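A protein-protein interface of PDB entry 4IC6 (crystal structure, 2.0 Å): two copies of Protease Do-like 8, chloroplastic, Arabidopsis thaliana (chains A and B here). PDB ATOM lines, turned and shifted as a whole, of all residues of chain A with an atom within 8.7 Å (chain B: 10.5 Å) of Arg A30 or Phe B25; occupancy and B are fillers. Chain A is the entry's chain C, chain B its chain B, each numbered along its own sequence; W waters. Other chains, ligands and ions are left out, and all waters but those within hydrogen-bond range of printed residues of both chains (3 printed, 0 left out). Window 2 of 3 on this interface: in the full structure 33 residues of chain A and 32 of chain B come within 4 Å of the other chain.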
ATOM      1  N   LEU A  24      31.867  -5.683  -3.969  1.00  0.00           N
ATOM      2  CA  LEU A  24      31.751  -6.100  -2.578  1.00  0.00           C
ATOM      3  C   LEU A  24      30.326  -6.539  -2.251  1.00  0.00           C
ATOM      4  O   LEU A  24      29.373  -6.133  -2.913  1.00  0.00           O
ATOM      5  CB  LEU A  24      32.164  -4.947  -1.658  1.00  0.00           C
ATOM      6  CG  LEU A  24      33.615  -4.451  -1.682  1.00  0.00           C
ATOM      7  CD1 LEU A  24      33.778  -3.253  -0.729  1.00  0.00           C
ATOM      8  CD2 LEU A  24      34.600  -5.564  -1.307  1.00  0.00           C
ATOM      9  N   PHE A  25      30.189  -7.379  -1.236  1.00  0.00           N
ATOM     10  CA  PHE A  25      28.871  -7.796  -0.774  1.00  0.00           C
ATOM     11  C   PHE A  25      28.240  -6.697   0.088  1.00  0.00           C
ATOM     12  O   PHE A  25      28.942  -5.770   0.525  1.00  0.00           O
ATOM     13  CB  PHE A  25      28.974  -9.157  -0.053  1.00  0.00           C
ATOM     14  CG  PHE A  25      29.281 -10.287  -0.992  1.00  0.00           C
ATOM     15  CD1 PHE A  25      28.289 -10.808  -1.804  1.00  0.00           C
ATOM     16  CD2 PHE A  25      30.566 -10.796  -1.106  1.00  0.00           C
ATOM     17  CE1 PHE A  25      28.563 -11.851  -2.696  1.00  0.00           C
ATOM     18  CE2 PHE A  25      30.848 -11.831  -1.997  1.00  0.00           C
ATOM     19  CZ  PHE A  25      29.844 -12.357  -2.791  1.00  0.00           C
ATOM     20  N   PRO A  26      26.919  -6.779   0.318  1.00  0.00           N
ATOM     21  CA  PRO A  26      26.178  -5.662   0.921  1.00  0.00           C
ATOM     22  C   PRO A  26      26.741  -5.158   2.240  1.00  0.00           C
ATOM     23  O   PRO A  26      27.032  -3.958   2.374  1.00  0.00           O
ATOM     24  CB  PRO A  26      24.779  -6.253   1.130  1.00  0.00           C
ATOM     25  CG  PRO A  26      24.645  -7.236  -0.035  1.00  0.00           C
ATOM     26  CD  PRO A  26      26.020  -7.888  -0.057  1.00  0.00           C
ATOM     27  N   THR A  27      26.903  -6.047   3.210  1.00  0.00           N
ATOM     28  CA  THR A  27      27.284  -5.591   4.544  1.00  0.00           C
ATOM     29  C   THR A  27      28.703  -5.017   4.542  1.00  0.00           C
ATOM     30  O   THR A  27      28.934  -3.911   5.054  1.00  0.00           O
ATOM     31  CB  THR A  27      27.143  -6.723   5.598  1.00  0.00           C
ATOM     32  OG1 THR A  27      25.768  -7.137   5.680  1.00  0.00           O
ATOM     33  CG2 THR A  27      27.614  -6.245   6.961  1.00  0.00           C
ATOM     34  N   GLU A  28      29.651  -5.744   3.942  1.00  0.00           N
ATOM     35  CA  GLU A  28      31.026  -5.248   3.902  1.00  0.00           C
ATOM     36  C   GLU A  28      31.094  -3.964   3.065  1.00  0.00           C
ATOM     37  O   GLU A  28      31.886  -3.067   3.367  1.00  0.00           O
ATOM     38  CB  GLU A  28      32.002  -6.306   3.346  1.00  0.00           C
ATOM     39  CG  GLU A  28      31.734  -6.654   1.873  1.00  0.00           C
ATOM     40  CD  GLU A  28      32.728  -7.655   1.302  1.00  0.00           C
ATOM     41  OE1 GLU A  28      33.802  -7.841   1.907  1.00  0.00           O
ATOM     42  OE2 GLU A  28      32.433  -8.260   0.236  1.00  0.00           O
ATOM     43  N   GLY A  29      30.273  -3.881   2.012  1.00  0.00           N
ATOM     44  CA  GLY A  29      30.193  -2.681   1.196  1.00  0.00           C
ATOM     45  C   GLY A  29      29.792  -1.471   2.040  1.00  0.00           C
ATOM     46  O   GLY A  29      30.381  -0.393   1.918  1.00  0.00           O
ATOM     47  N   ARG A  30      28.777  -1.648   2.885  1.00  0.00           N
ATOM     48  CA  ARG A  30      28.316  -0.583   3.777  1.00  0.00           C
ATOM     49  C   ARG A  30      29.376  -0.170   4.806  1.00  0.00           C
ATOM     50  O   ARG A  30      29.536   1.013   5.071  1.00  0.00           O
ATOM     51  CB  ARG A  30      26.985  -0.968   4.455  1.00  0.00           C
ATOM     52  CG  ARG A  30      25.777  -0.961   3.480  1.00  0.00           C
ATOM     53  CD  ARG A  30      24.402  -1.082   4.181  1.00  0.00           C
ATOM     54  NE  ARG A  30      24.167  -2.397   4.788  1.00  0.00           N
ATOM     55  CZ  ARG A  30      23.596  -3.434   4.168  1.00  0.00           C
ATOM     56  NH1 ARG A  30      23.201  -3.331   2.906  1.00  0.00           N
ATOM     57  NH2 ARG A  30      23.423  -4.585   4.814  1.00  0.00           N
ATOM     58  N   ILE A  31      30.118  -1.130   5.370  1.00  0.00           N
ATOM     59  CA  ILE A  31      31.179  -0.801   6.334  1.00  0.00           C
ATOM     60  C   ILE A  31      32.282  -0.002   5.654  1.00  0.00           C
ATOM     61  O   ILE A  31      32.753   1.018   6.161  1.00  0.00           O
ATOM     62  CB  ILE A  31      31.810  -2.074   6.929  1.00  0.00           C
ATOM     63  CG1 ILE A  31      30.734  -2.931   7.598  1.00  0.00           C
ATOM     64  CG2 ILE A  31      32.944  -1.715   7.908  1.00  0.00           C
ATOM     65  CD1 ILE A  31      31.290  -4.141   8.398  1.00  0.00           C
ATOM     66  N   VAL A  32      32.707  -0.480   4.493  1.00  0.00           N
ATOM     67  CA  VAL A  32      33.790   0.169   3.785  1.00  0.00           C
ATOM     68  C   VAL A  32      33.445   1.650   3.528  1.00  0.00           C
ATOM     69  O   VAL A  32      34.277   2.545   3.714  1.00  0.00           O
ATOM     70  CB  VAL A  32      34.060  -0.571   2.472  1.00  0.00           C
ATOM     71  CG1 VAL A  32      34.732   0.351   1.458  1.00  0.00           C
ATOM     72  CG2 VAL A  32      34.868  -1.857   2.736  1.00  0.00           C
ATOM     73  N   GLN A  33      32.214   1.903   3.115  1.00  0.00           N
ATOM     74  CA  GLN A  33      31.806   3.274   2.804  1.00  0.00           C
ATOM     75  C   GLN A  33      31.625   4.120   4.062  1.00  0.00           C
ATOM     76  O   GLN A  33      32.068   5.279   4.105  1.00  0.00           O
ATOM     77  CB  GLN A  33      30.569   3.287   1.887  1.00  0.00           C
ATOM     78  CG  GLN A  33      30.926   2.875   0.430  1.00  0.00           C
ATOM     79  CD  GLN A  33      29.709   2.674  -0.476  1.00  0.00           C
ATOM     80  OE1 GLN A  33      28.728   3.408  -0.386  1.00  0.00           O
ATOM     81  NE2 GLN A  33      29.777   1.667  -1.356  1.00  0.00           N
ATOM     82  N   LEU A  34      31.004   3.543   5.091  1.00  0.00           N
ATOM     83  CA  LEU A  34      30.842   4.225   6.389  1.00  0.00           C
ATOM     84  C   LEU A  34      32.176   4.632   6.976  1.00  0.00           C
ATOM     85  O   LEU A  34      32.336   5.753   7.466  1.00  0.00           O
ATOM     86  CB  LEU A  34      30.172   3.314   7.418  1.00  0.00           C
ATOM     87  CG  LEU A  34      28.763   3.631   7.899  1.00  0.00           C
ATOM     88  CD1 LEU A  34      28.605   3.068   9.302  1.00  0.00           C
ATOM     89  CD2 LEU A  34      28.447   5.134   7.849  1.00  0.00           C
ATOM     90  N   PHE A  35      33.127   3.699   6.953  1.00  0.00           N
ATOM     91  CA  PHE A  35      34.482   3.947   7.427  1.00  0.00           C
ATOM     92  C   PHE A  35      35.147   5.104   6.683  1.00  0.00           C
ATOM     93  O   PHE A  35      35.658   6.055   7.306  1.00  0.00           O
ATOM     94  CB  PHE A  35      35.346   2.680   7.288  1.00  0.00           C
ATOM     95  CG  PHE A  35      36.813   2.917   7.543  1.00  0.00           C
ATOM     96  CD1 PHE A  35      37.302   3.004   8.831  1.00  0.00           C
ATOM     97  CD2 PHE A  35      37.697   3.055   6.489  1.00  0.00           C
ATOM     98  CE1 PHE A  35      38.674   3.223   9.070  1.00  0.00           C
ATOM     99  CE2 PHE A  35      39.048   3.279   6.712  1.00  0.00           C
ATOM    100  CZ  PHE A  35      39.540   3.369   8.007  1.00  0.00           C
ATOM    101  N   GLU A  36      35.139   5.026   5.356  1.00  0.00           N
ATOM    102  CA  GLU A  36      35.785   6.050   4.530  1.00  0.00           C
ATOM    103  C   GLU A  36      35.196   7.420   4.814  1.00  0.00           C
ATOM    104  O   GLU A  36      35.916   8.408   5.007  1.00  0.00           O
ATOM    105  CB  GLU A  36      35.618   5.697   3.038  1.00  0.00           C
ATOM    106  CG  GLU A  36      35.902   6.828   2.080  1.00  0.00           C
ATOM    107  CD  GLU A  36      37.345   7.261   2.093  1.00  0.00           C
ATOM    108  OE1 GLU A  36      38.214   6.397   2.318  1.00  0.00           O
ATOM    109  OE2 GLU A  36      37.608   8.465   1.881  1.00  0.00           O
ATOM    110  N   LYS A  37      33.870   7.474   4.830  1.00  0.00           N
ATOM    111  CA  LYS A  37      33.153   8.720   5.040  1.00  0.00           C
ATOM    112  C   LYS A  37      33.541   9.330   6.390  1.00  0.00           C
ATOM    113  O   LYS A  37      33.615  10.539   6.523  1.00  0.00           O
ATOM    114  CB  LYS A  37      31.646   8.446   4.956  1.00  0.00           C
ATOM    115  CG  LYS A  37      30.730   9.611   5.276  1.00  0.00           C
ATOM    116  CD  LYS A  37      29.265   9.144   5.356  1.00  0.00           C
ATOM    117  CE  LYS A  37      28.308  10.334   5.470  1.00  0.00           C
ATOM    118  NZ  LYS A  37      26.905   9.925   5.808  1.00  0.00           N
ATOM    119  N   ASN A  38      33.838   8.494   7.378  1.00  0.00           N
ATOM    120  CA  ASN A  38      34.069   8.995   8.740  1.00  0.00           C
ATOM    121  C   ASN A  38      35.529   9.253   9.121  1.00  0.00           C
ATOM    122  O   ASN A  38      35.798   9.910  10.128  1.00  0.00           O
ATOM    123  CB  ASN A  38      33.374   8.098   9.777  1.00  0.00           C
ATOM    124  CG  ASN A  38      31.890   8.398   9.875  1.00  0.00           C
ATOM    125  OD1 ASN A  38      31.496   9.391  10.483  1.00  0.00           O
ATOM    126  ND2 ASN A  38      31.064   7.578   9.229  1.00  0.00           N
ATOM    127  N   GLY A 153      23.564  -6.160  20.598  1.00  0.00           N
ATOM    128  CA  GLY A 153      23.459  -6.896  19.355  1.00  0.00           C
ATOM    129  C   GLY A 153      23.688  -6.031  18.140  1.00  0.00           C
ATOM    130  O   GLY A 153      23.968  -6.551  17.051  1.00  0.00           O
ATOM    131  N   GLN A 154      23.587  -4.714  18.325  1.00  0.00           N
ATOM    132  CA  GLN A 154      23.818  -3.757  17.230  1.00  0.00           C
ATOM    133  C   GLN A 154      25.266  -3.767  16.738  1.00  0.00           C
ATOM    134  O   GLN A 154      26.206  -3.896  17.527  1.00  0.00           O
ATOM    135  CB  GLN A 154      23.545  -2.323  17.678  1.00  0.00           C
ATOM    136  CG  GLN A 154      22.128  -1.943  17.718  1.00  0.00           C
ATOM    137  CD  GLN A 154      21.977  -0.446  17.987  1.00  0.00           C
ATOM    138  OE1 GLN A 154      21.376  -0.039  18.996  1.00  0.00           O
ATOM    139  NE2 GLN A 154      22.546   0.386  17.082  1.00  0.00           N
ATOM    140  N   GLN A 155      25.430  -3.583  15.429  1.00  0.00           N
ATOM    141  CA  GLN A 155      26.752  -3.438  14.828  1.00  0.00           C
ATOM    142  C   GLN A 155      27.425  -2.166  15.343  1.00  0.00           C
ATOM    143  O   GLN A 155      26.789  -1.100  15.464  1.00  0.00           O
ATOM    144  CB  GLN A 155      26.636  -3.347  13.299  1.00  0.00           C
ATOM    145  CG  GLN A 155      27.962  -3.254  12.537  1.00  0.00           C
ATOM    146  CD  GLN A 155      27.726  -2.900  11.055  1.00  0.00           C
ATOM    147  OE1 GLN A 155      27.165  -1.852  10.748  1.00  0.00           O
ATOM    148  NE2 GLN A 155      28.132  -3.784  10.147  1.00  0.00           N
ATOM    149  N   LEU A 157      31.300   0.148  14.836  1.00  0.00           N
ATOM    150  CA  LEU A 157      32.582   0.359  14.200  1.00  0.00           C
ATOM    151  C   LEU A 157      33.412   1.212  15.109  1.00  0.00           C
ATOM    152  O   LEU A 157      32.974   2.294  15.499  1.00  0.00           O
ATOM    153  CB  LEU A 157      32.412   1.129  12.881  1.00  0.00           C
ATOM    154  CG  LEU A 157      31.336   0.774  11.855  1.00  0.00           C
ATOM    155  CD1 LEU A 157      31.810   1.271  10.482  1.00  0.00           C
ATOM    156  CD2 LEU A 157      31.017  -0.684  11.804  1.00  0.00           C
ATOM    157  N   LEU A 169      40.263   0.367  11.712  1.00  0.00           N
ATOM    158  CA  LEU A 169      38.888  -0.008  11.981  1.00  0.00           C
ATOM    159  C   LEU A 169      38.839  -1.344  12.678  1.00  0.00           C
ATOM    160  O   LEU A 169      39.575  -2.261  12.326  1.00  0.00           O
ATOM    161  CB  LEU A 169      38.151  -0.159  10.658  1.00  0.00           C
ATOM    162  CG  LEU A 169      36.741  -0.725  10.817  1.00  0.00           C
ATOM    163  CD1 LEU A 169      35.817   0.349  11.393  1.00  0.00           C
ATOM    164  CD2 LEU A 169      36.209  -1.170   9.463  1.00  0.00           C
ATOM    165  N   ASP A 210      27.620   3.605  15.300  1.00  0.00           N
ATOM    166  CA  ASP A 210      26.598   2.608  15.016  1.00  0.00           C
ATOM    167  C   ASP A 210      26.458   2.395  13.493  1.00  0.00           C
ATOM    168  O   ASP A 210      27.233   2.952  12.703  1.00  0.00           O
ATOM    169  CB  ASP A 210      25.256   2.977  15.680  1.00  0.00           C
ATOM    170  CG  ASP A 210      24.575   4.186  15.028  1.00  0.00           C
ATOM    171  OD1 ASP A 210      24.996   4.619  13.941  1.00  0.00           O
ATOM    172  OD2 ASP A 210      23.612   4.703  15.621  1.00  0.00           O
ATOM    173  N   SER A 211      25.487   1.595  13.071  1.00  0.00           N
ATOM    174  CA  SER A 211      25.409   1.226  11.649  1.00  0.00           C
ATOM    175  C   SER A 211      24.983   2.402  10.765  1.00  0.00           C
ATOM    176  O   SER A 211      25.035   2.304   9.540  1.00  0.00           O
ATOM    177  CB  SER A 211      24.469   0.041  11.427  1.00  0.00           C
ATOM    178  OG  SER A 211      23.154   0.327  11.897  1.00  0.00           O
ATOM    179  N   LYS A 212      24.549   3.500  11.384  1.00  0.00           N
ATOM    180  CA  LYS A 212      24.222   4.716  10.653  1.00  0.00           C
ATOM    181  C   LYS A 212      25.397   5.694  10.652  1.00  0.00           C
ATOM    182  O   LYS A 212      25.305   6.787  10.094  1.00  0.00           O
ATOM    183  CB  LYS A 212      22.984   5.377  11.258  1.00  0.00           C
ATOM    184  CG  LYS A 212      21.732   4.519  11.163  1.00  0.00           C
ATOM    185  CD  LYS A 212      21.425   4.164   9.707  1.00  0.00           C
ATOM    186  CE  LYS A 212      20.029   3.566   9.569  1.00  0.00           C
ATOM    187  NZ  LYS A 212      19.581   3.450   8.140  1.00  0.00           N
ATOM    188  N   GLY A 213      26.498   5.307  11.286  1.00  0.00           N
ATOM    189  CA  GLY A 213      27.663   6.168  11.334  1.00  0.00           C
ATOM    190  C   GLY A 213      27.495   7.277  12.368  1.00  0.00           C
ATOM    191  O   GLY A 213      28.185   8.293  12.331  1.00  0.00           O
ATOM    192  N   ALA B  21      17.530   6.617  17.506  1.00  0.00           N
ATOM    193  CA  ALA B  21      17.646   5.241  17.034  1.00  0.00           C
ATOM    194  C   ALA B  21      16.716   5.026  15.839  1.00  0.00           C
ATOM    195  O   ALA B  21      15.499   5.210  15.937  1.00  0.00           O
ATOM    196  CB  ALA B  21      17.320   4.259  18.147  1.00  0.00           C
ATOM    197  N   GLY B  22      17.300   4.656  14.703  1.00  0.00           N
ATOM    198  CA  GLY B  22      16.531   4.365  13.507  1.00  0.00           C
ATOM    199  C   GLY B  22      16.510   2.869  13.263  1.00  0.00           C
ATOM    200  O   GLY B  22      17.081   2.102  14.043  1.00  0.00           O
ATOM    201  N   PRO B  23      15.839   2.444  12.186  1.00  0.00           N
ATOM    202  CA  PRO B  23      15.788   1.021  11.848  1.00  0.00           C
ATOM    203  C   PRO B  23      17.183   0.406  11.708  1.00  0.00           C
ATOM    204  O   PRO B  23      18.157   1.075  11.353  1.00  0.00           O
ATOM    205  CB  PRO B  23      15.044   1.010  10.517  1.00  0.00           C
ATOM    206  CG  PRO B  23      14.103   2.194  10.637  1.00  0.00           C
ATOM    207  CD  PRO B  23      14.912   3.245  11.364  1.00  0.00           C
ATOM    208  N   LEU B  24      17.268  -0.878  12.021  1.00  0.00           N
ATOM    209  CA  LEU B  24      18.533  -1.594  12.017  1.00  0.00           C
ATOM    210  C   LEU B  24      18.659  -2.320  10.689  1.00  0.00           C
ATOM    211  O   LEU B  24      17.656  -2.600  10.036  1.00  0.00           O
ATOM    212  CB  LEU B  24      18.535  -2.600  13.164  1.00  0.00           C
ATOM    213  CG  LEU B  24      18.415  -1.949  14.550  1.00  0.00           C
ATOM    214  CD1 LEU B  24      18.398  -2.977  15.679  1.00  0.00           C
ATOM    215  CD2 LEU B  24      19.553  -0.968  14.751  1.00  0.00           C
ATOM    216  N   PHE B  25      19.881  -2.621  10.278  1.00  0.00           N
ATOM    217  CA  PHE B  25      20.075  -3.445   9.086  1.00  0.00           C
ATOM    218  C   PHE B  25      19.713  -4.907   9.363  1.00  0.00           C
ATOM    219  O   PHE B  25      19.610  -5.304  10.524  1.00  0.00           O
ATOM    220  CB  PHE B  25      21.487  -3.249   8.529  1.00  0.00           C
ATOM    221  CG  PHE B  25      21.690  -1.874   7.931  1.00  0.00           C
ATOM    222  CD1 PHE B  25      21.322  -1.611   6.618  1.00  0.00           C
ATOM    223  CD2 PHE B  25      22.195  -0.835   8.695  1.00  0.00           C
ATOM    224  CE1 PHE B  25      21.482  -0.329   6.063  1.00  0.00           C
ATOM    225  CE2 PHE B  25      22.357   0.448   8.149  1.00  0.00           C
ATOM    226  CZ  PHE B  25      22.003   0.692   6.830  1.00  0.00           C
ATOM    227  N   PRO B  26      19.474  -5.696   8.295  1.00  0.00           N
ATOM    228  CA  PRO B  26      18.937  -7.052   8.462  1.00  0.00           C
ATOM    229  C   PRO B  26      19.715  -7.924   9.436  1.00  0.00           C
ATOM    230  O   PRO B  26      19.121  -8.527  10.340  1.00  0.00           O
ATOM    231  CB  PRO B  26      19.012  -7.634   7.044  1.00  0.00           C
ATOM    232  CG  PRO B  26      18.770  -6.419   6.162  1.00  0.00           C
ATOM    233  CD  PRO B  26      19.559  -5.315   6.873  1.00  0.00           C
ATOM    234  N   THR B  27      21.024  -8.020   9.267  1.00  0.00           N
ATOM    235  CA  THR B  27      21.756  -8.965  10.094  1.00  0.00           C
ATOM    236  C   THR B  27      21.771  -8.546  11.560  1.00  0.00           C
ATOM    237  O   THR B  27      21.447  -9.355  12.444  1.00  0.00           O
ATOM    238  CB  THR B  27      23.177  -9.183   9.576  1.00  0.00           C
ATOM    239  OG1 THR B  27      23.097  -9.748   8.259  1.00  0.00           O
ATOM    240  CG2 THR B  27      23.915 -10.148  10.472  1.00  0.00           C
ATOM    241  N   GLU B  28      22.124  -7.287  11.829  1.00  0.00           N
ATOM    242  CA  GLU B  28      22.202  -6.837  13.219  1.00  0.00           C
ATOM    243  C   GLU B  28      20.796  -6.851  13.810  1.00  0.00           C
ATOM    244  O   GLU B  28      20.607  -7.131  14.998  1.00  0.00           O
ATOM    245  CB  GLU B  28      22.816  -5.436  13.330  1.00  0.00           C
ATOM    246  CG  GLU B  28      22.055  -4.379  12.507  1.00  0.00           C
ATOM    247  CD  GLU B  28      22.501  -2.926  12.760  1.00  0.00           C
ATOM    248  OE1 GLU B  28      23.249  -2.640  13.723  1.00  0.00           O
ATOM    249  OE2 GLU B  28      22.057  -2.052  11.994  1.00  0.00           O
ATOM    250  N   GLY B  29      19.804  -6.572  12.976  1.00  0.00           N
ATOM    251  CA  GLY B  29      18.419  -6.589  13.421  1.00  0.00           C
ATOM    252  C   GLY B  29      18.051  -7.958  13.971  1.00  0.00           C
ATOM    253  O   GLY B  29      17.434  -8.066  15.036  1.00  0.00           O
ATOM    254  N   ARG B  30      18.423  -9.006  13.241  1.00  0.00           N
ATOM    255  CA  ARG B  30      18.104 -10.379  13.644  1.00  0.00           C
ATOM    256  C   ARG B  30      18.822 -10.774  14.928  1.00  0.00           C
ATOM    257  O   ARG B  30      18.278 -11.495  15.760  1.00  0.00           O
ATOM    258  CB  ARG B  30      18.454 -11.359  12.517  1.00  0.00           C
ATOM    259  CG  ARG B  30      17.640 -11.142  11.230  1.00  0.00           C
ATOM    260  CD  ARG B  30      17.752 -12.361  10.329  1.00  0.00           C
ATOM    261  NE  ARG B  30      19.102 -12.905  10.389  1.00  0.00           N
ATOM    262  CZ  ARG B  30      20.016 -12.723   9.446  1.00  0.00           C
ATOM    263  NH1 ARG B  30      19.703 -12.032   8.352  1.00  0.00           N
ATOM    264  NH2 ARG B  30      21.233 -13.245   9.590  1.00  0.00           N
ATOM    265  N   ILE B  31      20.059 -10.319  15.069  1.00  0.00           N
ATOM    266  CA  ILE B  31      20.854 -10.592  16.272  1.00  0.00           C
ATOM    267  C   ILE B  31      20.221  -9.920  17.488  1.00  0.00           C
ATOM    268  O   ILE B  31      20.044 -10.545  18.540  1.00  0.00           O
ATOM    269  CB  ILE B  31      22.280 -10.068  16.105  1.00  0.00           C
ATOM    270  CG1 ILE B  31      23.017 -10.920  15.060  1.00  0.00           C
ATOM    271  CG2 ILE B  31      23.063 -10.093  17.450  1.00  0.00           C
ATOM    272  CD1 ILE B  31      24.414 -10.407  14.740  1.00  0.00           C
ATOM    273  N   VAL B  32      19.874  -8.642  17.337  1.00  0.00           N
ATOM    274  CA  VAL B  32      19.144  -7.908  18.374  1.00  0.00           C
ATOM    275  C   VAL B  32      17.905  -8.664  18.825  1.00  0.00           C
ATOM    276  O   VAL B  32      17.647  -8.786  20.029  1.00  0.00           O
ATOM    277  CB  VAL B  32      18.801  -6.473  17.878  1.00  0.00           C
ATOM    278  CG1 VAL B  32      17.633  -5.863  18.652  1.00  0.00           C
ATOM    279  CG2 VAL B  32      20.038  -5.605  17.990  1.00  0.00           C
ATOM    280  N   GLN B  33      17.143  -9.189  17.869  1.00  0.00           N
ATOM    281  CA  GLN B  33      15.911  -9.900  18.202  1.00  0.00           C
ATOM    282  C   GLN B  33      16.218 -11.232  18.868  1.00  0.00           C
ATOM    283  O   GLN B  33      15.559 -11.614  19.840  1.00  0.00           O
ATOM    284  CB  GLN B  33      15.038 -10.105  16.960  1.00  0.00           C
ATOM    285  N   GLN B 155      27.268 -18.520  11.935  1.00  0.00           N
ATOM    286  CA  GLN B 155      27.190 -17.480  12.957  1.00  0.00           C
ATOM    287  C   GLN B 155      26.873 -18.100  14.315  1.00  0.00           C
ATOM    288  O   GLN B 155      26.042 -19.011  14.408  1.00  0.00           O
ATOM    289  CB  GLN B 155      26.066 -16.501  12.588  1.00  0.00           C
ATOM    290  CG  GLN B 155      25.844 -15.347  13.555  1.00  0.00           C
ATOM    291  CD  GLN B 155      24.539 -14.599  13.225  1.00  0.00           C
ATOM    292  OE1 GLN B 155      23.461 -15.184  13.248  1.00  0.00           O
ATOM    293  NE2 GLN B 155      24.647 -13.318  12.907  1.00  0.00           N
HETATM  294  O   HOH W   1      25.445  -9.643   6.784  1.00  0.00           O
HETATM  295  O   HOH W   2      24.295  -3.065  10.088  1.00  0.00           O
HETATM  296  O   HOH W   3      24.228  -0.279  14.933  1.00  0.00           O
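The side-chain hydroxyl of Ser A211 is in hydrogen-bond range of the side-chain carboxylate of Glu B28, at 2.6 Å.
OE1 of Glu B28 sits at hydrogen-bond distance from N of Gln A155, 2.9 Å away.
The side-chain carboxylate of Asp A210 sits at hydrogen-bond distance from the backbone NH of Lys A212.
N of Phe B25 sits at hydrogen-bond distance from OE2 of Glu B28, 2.8 Å away.
Among the printed residues, merely in contact across the chains: Arg A30 with Phe B25 (3.5 Å), Ser A211 with Phe B25 (3.5 Å), Lys A212 with Pro B23 (3.6 Å), Gln A154 with Val B32 (3.7 Å), Gly A153 with Ile B31 (3.7 Å), Gly A153 with Val B32 (3.7 Å), Gln A154 with Glu B28 (3.7 Å), Lys A212 with Phe B25 (3.9 Å) and Gly A153 with Glu B28 (3.98 Å).
Of the printed residues of chain A, Phe B25 touches Arg A30 (3.5 Å), Ser A211 (3.5 Å) and Lys A212 (3.9 Å).
No residue of chain B comes within 4 Å of Pro A26.
No residue of chain B comes within 4 Å of Thr A27.
No residue of chain B comes within 4 Å of Gly A29.
Ile A31 touches none of the printed residues of chain B.
No residue of chain B comes within 4 Å of Val A32.
No residue of chain B comes within 4 Å of Leu A34.
Printed residues of chain B within 4 Å of Ser A211: Phe B25 and Glu B28.
Of the printed residues of chain A, Val B32 touches Gly A153 (3.7 Å) and Gln A154 (3.7 Å).
Of the printed residues of chain A, Ile B31 touches Gly A153 (3.7 Å).
The nearest residue of chain B that does not touch Arg A30 is Pro B26 (4.4 Å).
The nearest printed residue of chain B that does not touch Gln A154 is Leu B24 (4.03 Å).
Of the 24 printed residues of chain A, 6 touch a printed residue of chain B.
Of the 14 printed residues of chain B, 5 touch a printed residue of chain A.
Hydrophobic or aromatic side chains of chain B within 4 Å of the printed part of chain A: Phe B25, Ile B31 and Val B32.
Among the printed residues, 11 pairs touch across the chains.
Among the printed residues, no Asp or Glu carboxylate lies within 4 Å of a Lys or Arg side-chain nitrogen of the other chain.
Arg A30 touches Phe B25, but with the chains exchanged Phe A25 does not touch Arg B30 (12.8 Å).
Gln A155 touches Glu B28, but with the chains exchanged Glu A28 does not touch Gln B155 (12.8 Å).
11 positions are printed for both chains.
Water W3 lies within hydrogen-bond range of the backbone carbonyl oxygen of Gln A155 (2.7 Å), the side-chain amide nitrogen of Gln A154 (2.8 Å), the side-chain carboxylate of Glu B28 (2.8 Å) and the backbone NH of Ser A211 (2.9 Å).
Water W1 bridges OG1 of Thr A27 and OG1 of Thr B27.
Water W2 lies within hydrogen-bond range of OE2 of Glu B28 (3.1 Å) and OE1 of Gln A155 (3.2 Å).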
